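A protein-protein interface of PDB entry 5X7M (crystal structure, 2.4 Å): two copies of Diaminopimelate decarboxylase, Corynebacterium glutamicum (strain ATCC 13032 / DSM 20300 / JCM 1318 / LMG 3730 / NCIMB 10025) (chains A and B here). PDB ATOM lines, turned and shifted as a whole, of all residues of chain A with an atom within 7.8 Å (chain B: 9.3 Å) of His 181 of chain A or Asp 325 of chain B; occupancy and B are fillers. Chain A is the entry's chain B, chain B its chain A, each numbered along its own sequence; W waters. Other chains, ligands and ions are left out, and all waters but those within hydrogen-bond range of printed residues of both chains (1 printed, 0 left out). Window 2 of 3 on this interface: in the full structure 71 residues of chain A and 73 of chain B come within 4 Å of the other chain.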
ATOM      1  N   LYS A 166      -3.803 -13.551 -11.443  1.00  0.00           N
ATOM      2  CA  LYS A 166      -3.950 -13.638  -9.994  1.00  0.00           C
ATOM      3  C   LYS A 166      -2.682 -13.085  -9.348  1.00  0.00           C
ATOM      4  O   LYS A 166      -1.688 -13.804  -9.241  1.00  0.00           O
ATOM      5  CB  LYS A 166      -4.183 -15.089  -9.545  1.00  0.00           C
ATOM      6  CG  LYS A 166      -5.483 -15.698 -10.039  1.00  0.00           C
ATOM      7  CD  LYS A 166      -5.586 -17.186  -9.650  1.00  0.00           C
ATOM      8  CE  LYS A 166      -4.807 -18.095 -10.565  1.00  0.00           C
ATOM      9  NZ  LYS A 166      -5.330 -19.464 -10.411  1.00  0.00           N
ATOM     10  N   PRO A 167      -2.724 -11.829  -8.880  1.00  0.00           N
ATOM     11  CA  PRO A 167      -1.550 -11.220  -8.264  1.00  0.00           C
ATOM     12  C   PRO A 167      -1.269 -11.672  -6.831  1.00  0.00           C
ATOM     13  O   PRO A 167      -0.226 -11.332  -6.310  1.00  0.00           O
ATOM     14  CB  PRO A 167      -1.896  -9.728  -8.270  1.00  0.00           C
ATOM     15  CG  PRO A 167      -3.374  -9.705  -8.068  1.00  0.00           C
ATOM     16  CD  PRO A 167      -3.915 -10.982  -8.709  1.00  0.00           C
ATOM     17  N   GLY A 168      -2.191 -12.406  -6.201  1.00  0.00           N
ATOM     18  CA  GLY A 168      -2.047 -12.875  -4.819  1.00  0.00           C
ATOM     19  C   GLY A 168      -2.481 -11.865  -3.769  1.00  0.00           C
ATOM     20  O   GLY A 168      -1.835 -11.712  -2.742  1.00  0.00           O
ATOM     21  N   ILE A 169      -3.538 -11.144  -4.065  1.00  0.00           N
ATOM     22  CA  ILE A 169      -4.088 -10.146  -3.168  1.00  0.00           C
ATOM     23  C   ILE A 169      -5.603 -10.388  -3.125  1.00  0.00           C
ATOM     24  O   ILE A 169      -6.245 -10.598  -4.177  1.00  0.00           O
ATOM     25  CB  ILE A 169      -3.829  -8.714  -3.668  1.00  0.00           C
ATOM     26  CG1 ILE A 169      -2.318  -8.404  -3.733  1.00  0.00           C
ATOM     27  CG2 ILE A 169      -4.551  -7.711  -2.791  1.00  0.00           C
ATOM     28  CD1 ILE A 169      -1.586  -8.442  -2.401  1.00  0.00           C
ATOM     29  N   ALA A 178      -2.372 -11.167   1.551  1.00  0.00           N
ATOM     30  CA  ALA A 178      -1.407 -11.335   0.469  1.00  0.00           C
ATOM     31  C   ALA A 178      -0.729 -12.686   0.484  1.00  0.00           C
ATOM     32  O   ALA A 178      -0.202 -13.096   1.511  1.00  0.00           O
ATOM     33  CB  ALA A 178      -0.361 -10.234   0.514  1.00  0.00           C
ATOM     34  N   THR A 179      -0.722 -13.355  -0.663  1.00  0.00           N
ATOM     35  CA  THR A 179      -0.117 -14.657  -0.799  1.00  0.00           C
ATOM     36  C   THR A 179       0.742 -14.631  -2.043  1.00  0.00           C
ATOM     37  O   THR A 179       0.737 -13.662  -2.769  1.00  0.00           O
ATOM     38  CB  THR A 179      -1.204 -15.723  -0.949  1.00  0.00           C
ATOM     39  OG1 THR A 179      -2.034 -15.420  -2.081  1.00  0.00           O
ATOM     40  CG2 THR A 179      -2.096 -15.797   0.302  1.00  0.00           C
ATOM     41  N   SER A 180       1.511 -15.675  -2.257  1.00  0.00           N
ATOM     42  CA  SER A 180       2.125 -15.926  -3.571  1.00  0.00           C
ATOM     43  C   SER A 180       1.101 -16.292  -4.651  1.00  0.00           C
ATOM     44  O   SER A 180       1.152 -15.758  -5.732  1.00  0.00           O
ATOM     45  CB  SER A 180       3.117 -17.075  -3.493  1.00  0.00           C
ATOM     46  OG  SER A 180       4.317 -16.635  -2.895  1.00  0.00           O
ATOM     47  N   HIS A 181       0.195 -17.213  -4.341  1.00  0.00           N
ATOM     48  CA  HIS A 181      -0.742 -17.773  -5.300  1.00  0.00           C
ATOM     49  C   HIS A 181      -2.128 -17.720  -4.706  1.00  0.00           C
ATOM     50  O   HIS A 181      -2.276 -17.739  -3.465  1.00  0.00           O
ATOM     51  CB  HIS A 181      -0.401 -19.231  -5.573  1.00  0.00           C
ATOM     52  CG  HIS A 181       0.996 -19.455  -6.049  1.00  0.00           C
ATOM     53  ND1 HIS A 181       1.346 -19.432  -7.380  1.00  0.00           N
ATOM     54  CD2 HIS A 181       2.135 -19.710  -5.372  1.00  0.00           C
ATOM     55  CE1 HIS A 181       2.633 -19.693  -7.506  1.00  0.00           C
ATOM     56  NE2 HIS A 181       3.136 -19.862  -6.300  1.00  0.00           N
ATOM     57  N   GLU A 182      -3.139 -17.641  -5.574  1.00  0.00           N
ATOM     58  CA  GLU A 182      -4.528 -17.606  -5.132  1.00  0.00           C
ATOM     59  C   GLU A 182      -5.094 -18.948  -5.511  1.00  0.00           C
ATOM     60  O   GLU A 182      -5.106 -19.280  -6.689  1.00  0.00           O
ATOM     61  CB  GLU A 182      -5.339 -16.471  -5.772  1.00  0.00           C
ATOM     62  CG  GLU A 182      -4.891 -15.056  -5.431  1.00  0.00           C
ATOM     63  CD  GLU A 182      -5.664 -13.923  -6.153  1.00  0.00           C
ATOM     64  OE1 GLU A 182      -5.066 -12.870  -6.473  1.00  0.00           O
ATOM     65  OE2 GLU A 182      -6.880 -14.055  -6.411  1.00  0.00           O
ATOM     66  N   ASP A 183      -5.581 -19.705  -4.516  1.00  0.00           N
ATOM     67  CA  ASP A 183      -6.167 -21.039  -4.745  1.00  0.00           C
ATOM     68  C   ASP A 183      -7.614 -20.862  -5.199  1.00  0.00           C
ATOM     69  O   ASP A 183      -8.593 -21.029  -4.422  1.00  0.00           O
ATOM     70  CB  ASP A 183      -6.050 -21.930  -3.502  1.00  0.00           C
ATOM     71  CG  ASP A 183      -6.618 -23.345  -3.712  1.00  0.00           C
ATOM     72  OD1 ASP A 183      -6.978 -23.767  -4.833  1.00  0.00           O
ATOM     73  OD2 ASP A 183      -6.695 -24.083  -2.730  1.00  0.00           O
ATOM     74  N   GLN A 184      -7.753 -20.530  -6.475  1.00  0.00           N
ATOM     75  CA  GLN A 184      -9.088 -20.257  -7.020  1.00  0.00           C
ATOM     76  C   GLN A 184      -9.165 -20.392  -8.534  1.00  0.00           C
ATOM     77  O   GLN A 184      -8.163 -20.370  -9.213  1.00  0.00           O
ATOM     78  CB  GLN A 184      -9.614 -18.908  -6.491  1.00  0.00           C
ATOM     79  CG  GLN A 184      -8.657 -17.752  -6.668  1.00  0.00           C
ATOM     80  CD  GLN A 184      -9.080 -16.837  -7.783  1.00  0.00           C
ATOM     81  OE1 GLN A 184      -9.763 -17.263  -8.725  1.00  0.00           O
ATOM     82  NE2 GLN A 184      -8.703 -15.569  -7.683  1.00  0.00           N
ATOM     83  N   PHE A 188      -4.667 -16.804 -14.579  1.00  0.00           N
ATOM     84  CA  PHE A 188      -3.317 -17.382 -14.547  1.00  0.00           C
ATOM     85  C   PHE A 188      -2.575 -16.858 -13.312  1.00  0.00           C
ATOM     86  O   PHE A 188      -2.668 -15.675 -13.071  1.00  0.00           O
ATOM     87  CB  PHE A 188      -2.560 -16.917 -15.825  1.00  0.00           C
ATOM     88  CG  PHE A 188      -3.187 -17.395 -17.118  1.00  0.00           C
ATOM     89  CD1 PHE A 188      -4.221 -16.673 -17.712  1.00  0.00           C
ATOM     90  CD2 PHE A 188      -2.723 -18.515 -17.748  1.00  0.00           C
ATOM     91  CE1 PHE A 188      -4.847 -17.105 -18.870  1.00  0.00           C
ATOM     92  CE2 PHE A 188      -3.316 -18.943 -18.927  1.00  0.00           C
ATOM     93  CZ  PHE A 188      -4.398 -18.252 -19.473  1.00  0.00           C
ATOM     94  N   SER A 189      -1.829 -17.672 -12.559  1.00  0.00           N
ATOM     95  CA  SER A 189      -0.905 -17.096 -11.562  1.00  0.00           C
ATOM     96  C   SER A 189       0.118 -16.129 -12.133  1.00  0.00           C
ATOM     97  O   SER A 189       0.911 -16.468 -13.025  1.00  0.00           O
ATOM     98  CB  SER A 189      -0.092 -18.155 -10.826  1.00  0.00           C
ATOM     99  OG  SER A 189      -0.963 -18.931 -10.070  1.00  0.00           O
ATOM    100  N   LEU A 190       0.182 -14.965 -11.538  1.00  0.00           N
ATOM    101  CA  LEU A 190       1.370 -14.135 -11.656  1.00  0.00           C
ATOM    102  C   LEU A 190       2.659 -14.865 -11.270  1.00  0.00           C
ATOM    103  O   LEU A 190       3.586 -14.893 -12.046  1.00  0.00           O
ATOM    104  CB  LEU A 190       1.235 -12.883 -10.777  1.00  0.00           C
ATOM    105  CG  LEU A 190       2.280 -11.773 -10.933  1.00  0.00           C
ATOM    106  CD1 LEU A 190       2.009 -11.028 -12.227  1.00  0.00           C
ATOM    107  CD2 LEU A 190       2.262 -10.809  -9.747  1.00  0.00           C
ATOM    108  N   ALA A 191       2.704 -15.457 -10.086  1.00  0.00           N
ATOM    109  CA  ALA A 191       3.949 -15.955  -9.500  1.00  0.00           C
ATOM    110  C   ALA A 191       4.597 -17.202 -10.149  1.00  0.00           C
ATOM    111  O   ALA A 191       5.775 -17.370 -10.035  1.00  0.00           O
ATOM    112  CB  ALA A 191       3.748 -16.209  -8.024  1.00  0.00           C
ATOM    113  N   SER A 192       3.849 -18.080 -10.798  1.00  0.00           N
ATOM    114  CA  SER A 192       4.438 -19.230 -11.496  1.00  0.00           C
ATOM    115  C   SER A 192       4.968 -18.888 -12.903  1.00  0.00           C
ATOM    116  O   SER A 192       5.463 -19.779 -13.592  1.00  0.00           O
ATOM    117  CB  SER A 192       3.408 -20.369 -11.609  1.00  0.00           C
ATOM    118  OG  SER A 192       2.246 -19.960 -12.320  1.00  0.00           O
ATOM    119  N   GLY A 193       4.835 -17.630 -13.333  1.00  0.00           N
ATOM    120  CA  GLY A 193       5.139 -17.209 -14.696  1.00  0.00           C
ATOM    121  C   GLY A 193       4.050 -17.522 -15.722  1.00  0.00           C
ATOM    122  O   GLY A 193       4.220 -17.349 -16.923  1.00  0.00           O
ATOM    123  N   ARG A 233       2.011  -5.289  -8.260  1.00  0.00           N
ATOM    124  CA  ARG A 233       2.389  -6.611  -8.665  1.00  0.00           C
ATOM    125  C   ARG A 233       2.132  -6.870 -10.155  1.00  0.00           C
ATOM    126  O   ARG A 233       2.984  -7.451 -10.862  1.00  0.00           O
ATOM    127  CB  ARG A 233       1.666  -7.608  -7.771  1.00  0.00           C
ATOM    128  CG  ARG A 233       2.276  -7.674  -6.345  1.00  0.00           C
ATOM    129  CD  ARG A 233       1.508  -8.638  -5.475  1.00  0.00           C
ATOM    130  NE  ARG A 233       2.213  -8.907  -4.254  1.00  0.00           N
ATOM    131  CZ  ARG A 233       2.025  -9.961  -3.455  1.00  0.00           C
ATOM    132  NH1 ARG A 233       1.119 -10.940  -3.690  1.00  0.00           N
ATOM    133  NH2 ARG A 233       2.763 -10.032  -2.373  1.00  0.00           N
ATOM    134  N   ASP B 320      -4.290 -27.015 -13.944  1.00  0.00           N
ATOM    135  CA  ASP B 320      -3.550 -27.150 -12.713  1.00  0.00           C
ATOM    136  C   ASP B 320      -3.326 -25.750 -12.152  1.00  0.00           C
ATOM    137  O   ASP B 320      -2.814 -24.889 -12.831  1.00  0.00           O
ATOM    138  CB  ASP B 320      -2.242 -27.874 -12.966  1.00  0.00           C
ATOM    139  CG  ASP B 320      -2.461 -29.267 -13.567  1.00  0.00           C
ATOM    140  OD1 ASP B 320      -3.182 -30.097 -12.963  1.00  0.00           O
ATOM    141  OD2 ASP B 320      -1.911 -29.535 -14.648  1.00  0.00           O
ATOM    142  N   VAL B 321      -3.778 -25.512 -10.929  1.00  0.00           N
ATOM    143  CA  VAL B 321      -3.753 -24.191 -10.320  1.00  0.00           C
ATOM    144  C   VAL B 321      -2.724 -24.254  -9.187  1.00  0.00           C
ATOM    145  O   VAL B 321      -2.826 -25.103  -8.305  1.00  0.00           O
ATOM    146  CB  VAL B 321      -5.143 -23.862  -9.773  1.00  0.00           C
ATOM    147  CG1 VAL B 321      -5.130 -22.638  -8.893  1.00  0.00           C
ATOM    148  CG2 VAL B 321      -6.100 -23.672 -10.919  1.00  0.00           C
ATOM    149  N   HIS B 322      -1.728 -23.379  -9.233  1.00  0.00           N
ATOM    150  CA  HIS B 322      -0.707 -23.348  -8.191  1.00  0.00           C
ATOM    151  C   HIS B 322      -1.344 -22.837  -6.907  1.00  0.00           C
ATOM    152  O   HIS B 322      -2.110 -21.899  -6.950  1.00  0.00           O
ATOM    153  CB  HIS B 322       0.498 -22.497  -8.614  1.00  0.00           C
ATOM    154  CG  HIS B 322       1.365 -23.149  -9.646  1.00  0.00           C
ATOM    155  ND1 HIS B 322       2.399 -24.007  -9.317  1.00  0.00           N
ATOM    156  CD2 HIS B 322       1.344 -23.083 -10.999  1.00  0.00           C
ATOM    157  CE1 HIS B 322       2.979 -24.436 -10.421  1.00  0.00           C
ATOM    158  NE2 HIS B 322       2.359 -23.890 -11.455  1.00  0.00           N
ATOM    159  N   VAL B 323      -1.087 -23.528  -5.803  1.00  0.00           N
ATOM    160  CA  VAL B 323      -1.549 -23.133  -4.466  1.00  0.00           C
ATOM    161  C   VAL B 323      -0.379 -22.681  -3.564  1.00  0.00           C
ATOM    162  O   VAL B 323      -0.595 -21.926  -2.634  1.00  0.00           O
ATOM    163  CB  VAL B 323      -2.391 -24.234  -3.783  1.00  0.00           C
ATOM    164  CG1 VAL B 323      -3.590 -24.603  -4.651  1.00  0.00           C
ATOM    165  CG2 VAL B 323      -1.576 -25.483  -3.471  1.00  0.00           C
ATOM    166  N   ASP B 324       0.829 -23.195  -3.808  1.00  0.00           N
ATOM    167  CA  ASP B 324       2.071 -22.473  -3.519  1.00  0.00           C
ATOM    168  C   ASP B 324       3.101 -22.842  -4.602  1.00  0.00           C
ATOM    169  O   ASP B 324       2.693 -23.290  -5.665  1.00  0.00           O
ATOM    170  CB  ASP B 324       2.552 -22.597  -2.040  1.00  0.00           C
ATOM    171  CG  ASP B 324       2.617 -24.033  -1.533  1.00  0.00           C
ATOM    172  OD1 ASP B 324       2.972 -24.949  -2.321  1.00  0.00           O
ATOM    173  OD2 ASP B 324       2.333 -24.218  -0.312  1.00  0.00           O
ATOM    174  N   ASP B 325       4.399 -22.649  -4.368  1.00  0.00           N
ATOM    175  CA  ASP B 325       5.398 -22.715  -5.453  1.00  0.00           C
ATOM    176  C   ASP B 325       5.518 -24.071  -6.145  1.00  0.00           C
ATOM    177  O   ASP B 325       5.785 -24.124  -7.348  1.00  0.00           O
ATOM    178  CB  ASP B 325       6.795 -22.253  -4.971  1.00  0.00           C
ATOM    179  CG  ASP B 325       6.884 -20.737  -4.790  1.00  0.00           C
ATOM    180  OD1 ASP B 325       6.821 -20.022  -5.800  1.00  0.00           O
ATOM    181  OD2 ASP B 325       7.017 -20.252  -3.644  1.00  0.00           O
ATOM    182  N   ASP B 326       5.302 -25.143  -5.389  1.00  0.00           N
ATOM    183  CA  ASP B 326       5.602 -26.502  -5.837  1.00  0.00           C
ATOM    184  C   ASP B 326       4.381 -27.434  -5.867  1.00  0.00           C
ATOM    185  O   ASP B 326       4.509 -28.603  -6.227  1.00  0.00           O
ATOM    186  CB  ASP B 326       6.712 -27.100  -4.939  1.00  0.00           C
ATOM    187  CG  ASP B 326       6.409 -26.980  -3.413  1.00  0.00           C
ATOM    188  OD1 ASP B 326       5.260 -27.241  -2.981  1.00  0.00           O
ATOM    189  OD2 ASP B 326       7.333 -26.631  -2.639  1.00  0.00           O
ATOM    190  N   LYS B 327       3.204 -26.909  -5.520  1.00  0.00           N
ATOM    191  CA  LYS B 327       2.026 -27.713  -5.176  1.00  0.00           C
ATOM    192  C   LYS B 327       0.842 -27.214  -6.022  1.00  0.00           C
ATOM    193  O   LYS B 327       0.604 -26.001  -6.080  1.00  0.00           O
ATOM    194  CB  LYS B 327       1.753 -27.526  -3.688  1.00  0.00           C
ATOM    195  CG  LYS B 327       1.167 -28.720  -2.970  1.00  0.00           C
ATOM    196  CD  LYS B 327       0.982 -28.420  -1.479  1.00  0.00           C
ATOM    197  CE  LYS B 327       0.115 -29.468  -0.775  1.00  0.00           C
ATOM    198  NZ  LYS B 327      -0.877 -28.869   0.164  1.00  0.00           N
ATOM    199  N   THR B 328       0.138 -28.117  -6.718  1.00  0.00           N
ATOM    200  CA  THR B 328      -0.989 -27.707  -7.569  1.00  0.00           C
ATOM    201  C   THR B 328      -2.298 -28.385  -7.198  1.00  0.00           C
ATOM    202  O   THR B 328      -2.334 -29.331  -6.454  1.00  0.00           O
ATOM    203  CB  THR B 328      -0.749 -27.870  -9.097  1.00  0.00           C
ATOM    204  OG1 THR B 328      -0.872 -29.238  -9.477  1.00  0.00           O
ATOM    205  CG2 THR B 328       0.587 -27.347  -9.523  1.00  0.00           C
HETATM  206  O   HOH W   1       4.583 -19.968  -2.093  1.00  0.00           O
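The backbone carbonyl oxygen (O) of Lys 166 of chain A lies within hydrogen-bond range of the backbone NH (N) of Leu 190 of chain A.
The side-chain carboxylate of Glu 182 of chain A is in hydrogen-bond range of the side-chain amide nitrogen of Gln 184 of chain A, at 2.7 Å.
The side-chain hydroxyl of Thr 179 of chain A sits at hydrogen-bond distance from the backbone carbonyl oxygen of His 181 of chain A, 2.7 Å away.
The backbone NH (N) of Lys 166 of chain A is in hydrogen-bond range of the backbone carbonyl oxygen (O) of Phe 188 of chain A, at 2.9 Å.
The backbone NH (N) of Ile 169 of chain A is in hydrogen-bond range of the side-chain carboxylate (OE1) of Glu 182 of chain A, 3.3 Å away.
The side-chain amino group (NZ) of Lys 166 of chain A sits at hydrogen-bond distance from the backbone carbonyl oxygen (O) of Gln 184 of chain A (3.2 Å).
Among the printed residues, merely in contact across the chains: His 181 of chain A with Asp 324 of chain B (3.3 Å), Asp 183 of chain A with Val 323 of chain B (3.4 Å), His 181 of chain A with His 322 of chain B (3.4 Å), Ser 192 of chain A with His 322 of chain B (3.5 Å), Lys 166 of chain A with Val 321 of chain B (3.5 Å), His 181 of chain A with Asp 325 of chain B (3.6 Å), Gln 184 of chain A with Val 321 of chain B (3.8 Å), Glu 182 of chain A with His 322 of chain B (3.99 Å) and His 181 of chain A with Val 323 of chain B (3.99 Å).
Ser 180 of chain A touches none of the printed residues of chain B.
Of the printed residues of chain B, His 181 of chain A touches His 322 (3.4 Å), Val 323 (3.99 Å), Asp 324 (3.3 Å) and Asp 325 (3.6 Å).
Of the printed residues of chain B, Glu 182 of chain A touches His 322 (3.99 Å).
Printed residues of chain B within 4 Å of Asp 183 of chain A: Val 323 (3.4 Å).
Phe 188 of chain A touches none of the printed residues of chain B.
Leu 190 of chain A touches none of the printed residues of chain B.
Printed residues of chain A within 4 Å of Asp 325 of chain B: His 181 (3.6 Å).
The nearest residue of chain A that does not touch Asp 325 of chain B is Ser 180 of chain A (4.6 Å).
The nearest printed residue of chain A that does not touch Asp 324 of chain B is Ser 180 of chain A (5.5 Å).
Of the 18 printed residues of chain A, 6 touch a printed residue of chain B.
Hydrophobic or aromatic side chains of chain A within 4 Å of the printed part of chain B: His 181.
Hydrophobic or aromatic side chains of chain B that line the printed part of chain A: Val 321, His 322 and Val 323.
Among the printed residues, 9 pairs touch across the chains.
Among the printed residues, no Asp or Glu carboxylate lies within 4 Å of a Lys or Arg side-chain nitrogen of the other chain.
No position is printed for both chains.
Water W1 lies within hydrogen-bond range of the side-chain carboxylate of Asp 325 of chain B (2.9 Å) and the side-chain hydroxyl of Ser 180 of chain A (3.4 Å).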
